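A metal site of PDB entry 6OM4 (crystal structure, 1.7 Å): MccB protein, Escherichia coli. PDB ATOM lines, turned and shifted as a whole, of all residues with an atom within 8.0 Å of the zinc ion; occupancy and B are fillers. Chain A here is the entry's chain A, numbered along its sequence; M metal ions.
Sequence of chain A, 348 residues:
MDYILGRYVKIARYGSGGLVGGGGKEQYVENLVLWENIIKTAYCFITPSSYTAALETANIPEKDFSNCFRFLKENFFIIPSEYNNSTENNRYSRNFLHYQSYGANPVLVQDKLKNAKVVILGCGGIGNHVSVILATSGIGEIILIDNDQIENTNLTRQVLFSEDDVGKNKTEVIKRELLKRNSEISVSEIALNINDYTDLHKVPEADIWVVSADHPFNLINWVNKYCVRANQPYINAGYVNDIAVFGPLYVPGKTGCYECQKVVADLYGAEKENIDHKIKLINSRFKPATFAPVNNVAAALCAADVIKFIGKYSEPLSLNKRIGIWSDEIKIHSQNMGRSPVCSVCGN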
ATOM      1  N   ASN A 224     -32.956 -23.930  28.802  1.00  0.00           N
ATOM      2  CA  ASN A 224     -31.871 -23.016  28.826  1.00  0.00           C
ATOM      3  C   ASN A 224     -32.229 -21.838  29.744  1.00  0.00           C
ATOM      4  O   ASN A 224     -31.464 -21.497  30.655  1.00  0.00           O
ATOM      5  CB  ASN A 224     -31.529 -22.582  27.415  1.00  0.00           C
ATOM      6  CG  ASN A 224     -30.420 -21.546  27.358  1.00  0.00           C
ATOM      7  OD1 ASN A 224     -30.647 -20.348  27.136  1.00  0.00           O
ATOM      8  ND2 ASN A 224     -29.233 -22.006  27.642  1.00  0.00           N
ATOM      9  N   VAL A 228     -30.432 -21.025  33.372  1.00  0.00           N
ATOM     10  CA  VAL A 228     -29.752 -19.740  33.629  1.00  0.00           C
ATOM     11  C   VAL A 228     -30.343 -19.114  34.891  1.00  0.00           C
ATOM     12  O   VAL A 228     -29.604 -18.627  35.780  1.00  0.00           O
ATOM     13  CB  VAL A 228     -29.884 -18.803  32.413  1.00  0.00           C
ATOM     14  CG1 VAL A 228     -29.423 -17.402  32.757  1.00  0.00           C
ATOM     15  CG2 VAL A 228     -29.107 -19.294  31.194  1.00  0.00           C
ATOM     16  N   TYR A 250     -23.648 -26.129  29.575  1.00  0.00           N
ATOM     17  CA  TYR A 250     -23.901 -24.811  30.168  1.00  0.00           C
ATOM     18  C   TYR A 250     -23.469 -24.867  31.629  1.00  0.00           C
ATOM     19  O   TYR A 250     -23.982 -25.673  32.404  1.00  0.00           O
ATOM     20  CB  TYR A 250     -25.383 -24.432  30.103  1.00  0.00           C
ATOM     21  CG  TYR A 250     -25.690 -23.221  30.950  1.00  0.00           C
ATOM     22  CD1 TYR A 250     -25.117 -22.006  30.622  1.00  0.00           C
ATOM     23  CD2 TYR A 250     -26.411 -23.313  32.126  1.00  0.00           C
ATOM     24  CE1 TYR A 250     -25.314 -20.893  31.414  1.00  0.00           C
ATOM     25  CE2 TYR A 250     -26.670 -22.188  32.898  1.00  0.00           C
ATOM     26  CZ  TYR A 250     -26.073 -20.992  32.563  1.00  0.00           C
ATOM     27  OH  TYR A 250     -26.273 -19.867  33.342  1.00  0.00           O
ATOM     28  N   THR A 255     -19.772 -20.517  30.961  1.00  0.00           N
ATOM     29  CA  THR A 255     -19.877 -20.746  29.550  1.00  0.00           C
ATOM     30  C   THR A 255     -21.023 -19.941  28.960  1.00  0.00           C
ATOM     31  O   THR A 255     -21.850 -19.375  29.692  1.00  0.00           O
ATOM     32  CB  THR A 255     -20.124 -22.219  29.222  1.00  0.00           C
ATOM     33  OG1 THR A 255     -21.379 -22.573  29.807  1.00  0.00           O
ATOM     34  CG2 THR A 255     -19.018 -23.119  29.723  1.00  0.00           C
ATOM     35  N   GLY A 256     -21.073 -19.918  27.621  1.00  0.00           N
ATOM     36  CA  GLY A 256     -22.247 -19.401  26.934  1.00  0.00           C
ATOM     37  C   GLY A 256     -23.463 -20.257  27.181  1.00  0.00           C
ATOM     38  O   GLY A 256     -23.345 -21.431  27.598  1.00  0.00           O
ATOM     39  N   CYS A 257     -24.641 -19.681  26.942  1.00  0.00           N
ATOM     40  CA  CYS A 257     -25.888 -20.431  26.960  1.00  0.00           C
ATOM     41  C   CYS A 257     -26.306 -20.713  25.505  1.00  0.00           C
ATOM     42  O   CYS A 257     -25.647 -20.288  24.563  1.00  0.00           O
ATOM     43  CB  CYS A 257     -26.972 -19.717  27.764  1.00  0.00           C
ATOM     44  SG  CYS A 257     -27.813 -18.411  26.859  1.00  0.00           S
ATOM     45  N   TYR A 258     -27.396 -21.466  25.341  1.00  0.00           N
ATOM     46  CA  TYR A 258     -27.906 -21.857  24.029  1.00  0.00           C
ATOM     47  C   TYR A 258     -28.223 -20.659  23.122  1.00  0.00           C
ATOM     48  O   TYR A 258     -28.142 -20.786  21.905  1.00  0.00           O
ATOM     49  CB  TYR A 258     -29.139 -22.728  24.228  1.00  0.00           C
ATOM     50  CG  TYR A 258     -29.567 -23.524  23.014  1.00  0.00           C
ATOM     51  CD1 TYR A 258     -28.930 -24.699  22.657  1.00  0.00           C
ATOM     52  CD2 TYR A 258     -30.656 -23.126  22.268  1.00  0.00           C
ATOM     53  CE1 TYR A 258     -29.355 -25.453  21.567  1.00  0.00           C
ATOM     54  CE2 TYR A 258     -31.099 -23.869  21.177  1.00  0.00           C
ATOM     55  CZ  TYR A 258     -30.456 -25.051  20.851  1.00  0.00           C
ATOM     56  OH  TYR A 258     -30.932 -25.769  19.776  1.00  0.00           O
ATOM     57  N   GLU A 259     -28.495 -19.487  23.719  1.00  0.00           N
ATOM     58  CA  GLU A 259     -28.959 -18.298  22.925  1.00  0.00           C
ATOM     59  C   GLU A 259     -27.865 -17.224  22.789  1.00  0.00           C
ATOM     60  O   GLU A 259     -28.051 -16.242  22.079  1.00  0.00           O
ATOM     61  CB  GLU A 259     -30.251 -17.774  23.557  1.00  0.00           C
ATOM     62  CG  GLU A 259     -31.327 -18.838  23.453  1.00  0.00           C
ATOM     63  CD  GLU A 259     -32.764 -18.411  23.355  1.00  0.00           C
ATOM     64  OE1 GLU A 259     -33.035 -17.220  23.044  1.00  0.00           O
ATOM     65  OE2 GLU A 259     -33.607 -19.268  23.634  1.00  0.00           O
ATOM     66  N   CYS A 260     -26.699 -17.443  23.387  1.00  0.00           N
ATOM     67  CA  CYS A 260     -25.669 -16.398  23.353  1.00  0.00           C
ATOM     68  C   CYS A 260     -25.305 -16.048  21.909  1.00  0.00           C
ATOM     69  O   CYS A 260     -25.268 -14.864  21.543  1.00  0.00           O
ATOM     70  CB  CYS A 260     -24.388 -16.834  24.057  1.00  0.00           C
ATOM     71  SG  CYS A 260     -24.394 -16.558  25.843  1.00  0.00           S
ATOM     72  N   GLN A 261     -25.011 -17.082  21.105  1.00  0.00           N
ATOM     73  CA  GLN A 261     -24.641 -16.905  19.710  1.00  0.00           C
ATOM     74  C   GLN A 261     -25.814 -17.381  18.861  1.00  0.00           C
ATOM     75  O   GLN A 261     -26.541 -18.283  19.258  1.00  0.00           O
ATOM     76  CB  GLN A 261     -23.366 -17.661  19.359  1.00  0.00           C
ATOM     77  CG  GLN A 261     -22.270 -17.491  20.385  1.00  0.00           C
ATOM     78  CD  GLN A 261     -21.666 -16.118  20.276  1.00  0.00           C
ATOM     79  OE1 GLN A 261     -21.612 -15.548  19.187  1.00  0.00           O
ATOM     80  NE2 GLN A 261     -21.205 -15.587  21.395  1.00  0.00           N
ATOM     81  N   LYS A 262     -25.962 -16.787  17.694  1.00  0.00           N
ATOM     82  CA  LYS A 262     -27.203 -16.937  16.948  1.00  0.00           C
ATOM     83  C   LYS A 262     -26.948 -17.830  15.743  1.00  0.00           C
ATOM     84  O   LYS A 262     -27.034 -17.380  14.596  1.00  0.00           O
ATOM     85  CB  LYS A 262     -27.750 -15.549  16.615  1.00  0.00           C
ATOM     86  CG  LYS A 262     -27.861 -14.668  17.846  1.00  0.00           C
ATOM     87  CD  LYS A 262     -28.583 -13.347  17.671  1.00  0.00           C
ATOM     88  CE  LYS A 262     -28.620 -12.548  18.958  1.00  0.00           C
ATOM     89  NZ  LYS A 262     -28.958 -13.412  20.129  1.00  0.00           N
ATOM     90  N   MET A 337     -20.635 -21.452  20.926  1.00  0.00           N
ATOM     91  CA  MET A 337     -21.633 -20.940  21.864  1.00  0.00           C
ATOM     92  C   MET A 337     -20.933 -20.314  23.093  1.00  0.00           C
ATOM     93  O   MET A 337     -21.318 -20.534  24.241  1.00  0.00           O
ATOM     94  CB  MET A 337     -22.587 -22.050  22.300  1.00  0.00           C
ATOM     95  CG  MET A 337     -23.487 -22.549  21.154  1.00  0.00           C
ATOM     96  SD  MET A 337     -24.852 -23.536  21.746  1.00  0.00           S
ATOM     97  CE  MET A 337     -25.919 -23.454  20.311  1.00  0.00           C
ATOM     98  N   GLY A 338     -19.874 -19.540  22.843  1.00  0.00           N
ATOM     99  CA  GLY A 338     -19.221 -18.749  23.892  1.00  0.00           C
ATOM    100  C   GLY A 338     -20.123 -17.650  24.424  1.00  0.00           C
ATOM    101  O   GLY A 338     -21.113 -17.246  23.805  1.00  0.00           O
ATOM    102  N   ARG A 339     -19.774 -17.140  25.605  1.00  0.00           N
ATOM    103  CA  ARG A 339     -20.603 -16.163  26.315  1.00  0.00           C
ATOM    104  C   ARG A 339     -20.675 -14.880  25.500  1.00  0.00           C
ATOM    105  O   ARG A 339     -19.637 -14.424  25.005  1.00  0.00           O
ATOM    106  CB  ARG A 339     -20.025 -15.824  27.688  1.00  0.00           C
ATOM    107  CG  ARG A 339     -20.446 -16.775  28.790  1.00  0.00           C
ATOM    108  CD  ARG A 339     -20.336 -16.144  30.170  1.00  0.00           C
ATOM    109  NE  ARG A 339     -21.456 -15.260  30.464  1.00  0.00           N
ATOM    110  CZ  ARG A 339     -21.696 -14.800  31.675  1.00  0.00           C
ATOM    111  NH1 ARG A 339     -20.766 -14.951  32.599  1.00  0.00           N
ATOM    112  NH2 ARG A 339     -22.841 -14.202  31.974  1.00  0.00           N
ATOM    113  N   SER A 340     -21.872 -14.294  25.394  1.00  0.00           N
ATOM    114  CA  SER A 340     -22.015 -12.937  24.823  1.00  0.00           C
ATOM    115  C   SER A 340     -22.388 -11.999  25.951  1.00  0.00           C
ATOM    116  O   SER A 340     -23.325 -12.317  26.666  1.00  0.00           O
ATOM    117  CB  SER A 340     -23.053 -12.870  23.729  1.00  0.00           C
ATOM    118  OG  SER A 340     -23.326 -11.520  23.371  1.00  0.00           O
ATOM    119  N   PRO A 341     -21.719 -10.841  26.114  1.00  0.00           N
ATOM    120  CA  PRO A 341     -22.077  -9.872  27.163  1.00  0.00           C
ATOM    121  C   PRO A 341     -23.444  -9.200  26.922  1.00  0.00           C
ATOM    122  O   PRO A 341     -24.039  -8.577  27.835  1.00  0.00           O
ATOM    123  CB  PRO A 341     -20.924  -8.843  27.095  1.00  0.00           C
ATOM    124  CG  PRO A 341     -20.438  -8.920  25.671  1.00  0.00           C
ATOM    125  CD  PRO A 341     -20.603 -10.370  25.263  1.00  0.00           C
ATOM    126  N   VAL A 342     -23.976  -9.439  25.719  1.00  0.00           N
ATOM    127  CA  VAL A 342     -25.204  -8.871  25.187  1.00  0.00           C
ATOM    128  C   VAL A 342     -26.288  -9.956  25.028  1.00  0.00           C
ATOM    129  O   VAL A 342     -27.357  -9.754  24.418  1.00  0.00           O
ATOM    130  CB  VAL A 342     -24.724  -8.180  23.885  1.00  0.00           C
ATOM    131  CG1 VAL A 342     -25.308  -8.724  22.601  1.00  0.00           C
ATOM    132  CG2 VAL A 342     -24.817  -6.675  24.007  1.00  0.00           C
ATOM    133  N   CYS A 343     -26.055 -11.150  25.599  1.00  0.00           N
ATOM    134  CA  CYS A 343     -27.059 -12.225  25.535  1.00  0.00           C
ATOM    135  C   CYS A 343     -28.320 -11.769  26.264  1.00  0.00           C
ATOM    136  O   CYS A 343     -28.240 -11.372  27.422  1.00  0.00           O
ATOM    137  CB  CYS A 343     -26.578 -13.544  26.153  1.00  0.00           C
ATOM    138  SG  CYS A 343     -27.824 -14.851  26.001  1.00  0.00           S
ATOM    139  N   SER A 344     -29.480 -11.815  25.602  1.00  0.00           N
ATOM    140  CA  SER A 344     -30.722 -11.380  26.252  1.00  0.00           C
ATOM    141  C   SER A 344     -31.111 -12.329  27.393  1.00  0.00           C
ATOM    142  O   SER A 344     -31.897 -11.965  28.242  1.00  0.00           O
ATOM    143  CB  SER A 344     -31.839 -11.236  25.257  1.00  0.00           C
ATOM    144  OG  SER A 344     -32.139 -12.506  24.691  1.00  0.00           O
ATOM    145  N   VAL A 345     -30.564 -13.557  27.401  1.00  0.00           N
ATOM    146  CA  VAL A 345     -30.902 -14.515  28.449  1.00  0.00           C
ATOM    147  C   VAL A 345     -29.913 -14.420  29.622  1.00  0.00           C
ATOM    148  O   VAL A 345     -30.323 -14.269  30.727  1.00  0.00           O
ATOM    149  CB  VAL A 345     -31.006 -15.944  27.899  1.00  0.00           C
ATOM    150  CG1 VAL A 345     -31.352 -16.945  28.999  1.00  0.00           C
ATOM    151  CG2 VAL A 345     -32.053 -16.008  26.795  1.00  0.00           C
ATOM    152  N   CYS A 346     -28.608 -14.565  29.354  1.00  0.00           N
ATOM    153  CA  CYS A 346     -27.650 -14.823  30.403  1.00  0.00           C
ATOM    154  C   CYS A 346     -26.655 -13.650  30.588  1.00  0.00           C
ATOM    155  O   CYS A 346     -25.857 -13.677  31.479  1.00  0.00           O
ATOM    156  CB  CYS A 346     -26.922 -16.146  30.126  1.00  0.00           C
ATOM    157  SG  CYS A 346     -25.607 -16.039  28.886  1.00  0.00           S
ATOM    158  N   GLY A 347     -26.726 -12.613  29.768  1.00  0.00           N
ATOM    159  CA  GLY A 347     -25.802 -11.490  29.865  1.00  0.00           C
ATOM    160  C   GLY A 347     -25.650 -10.992  31.305  1.00  0.00           C
ATOM    161  O   GLY A 347     -26.627 -10.880  32.026  1.00  0.00           O
ATOM    162  N   ASN A 348     -24.393 -10.718  31.683  1.00  0.00           N
ATOM    163  CA  ASN A 348     -23.898 -10.272  33.025  1.00  0.00           C
ATOM    164  C   ASN A 348     -24.812 -10.734  34.173  1.00  0.00           C
ATOM    165  O   ASN A 348     -24.615 -10.338  35.335  1.00  0.00           O
ATOM    166  CB  ASN A 348     -23.655  -8.757  33.035  1.00  0.00           C
ATOM    167  CG  ASN A 348     -22.469  -8.383  32.171  1.00  0.00           C
ATOM    168  OD1 ASN A 348     -21.320  -8.750  32.486  1.00  0.00           O
ATOM    169  ND2 ASN A 348     -22.735  -7.723  31.057  1.00  0.00           N
HETATM  170 ZN    ZN M   1     -26.522 -16.574  26.774  1.00  0.00          ZN
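The side-chain sulfur of Cys 257 sits close to the backbone NH of Glu 259, at 3.4 Å. The side-chain sulfur (SG) of Cys 257 lies close to the side-chain amide oxygen (OD1) of Asn 224 (3.4 Å). The side-chain sulfur (SG) of Cys 343 sits close to the backbone NH (N) of Val 345, at 3.3 Å. The side-chain sulfur of Cys 260 sits close to the backbone NH of Ser 340 (3.4 Å). The backbone carbonyl oxygen of Cys 346 sits at hydrogen-bond distance from the guanidinium group of Arg 339, at 3.1 Å.
Four residues have an atom within 4 Å of the zinc ion: Cys 257, Cys 260, Cys 343 and Cys 346.
The zinc ion is bound by SG of Cys 257 (2.2 Å). SG of Cys 343 binds the zinc ion (2.3 Å). SG of Cys 260 is bound to the zinc ion (2.3 Å). SG of Cys 346 is bound to the zinc ion (2.4 Å).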
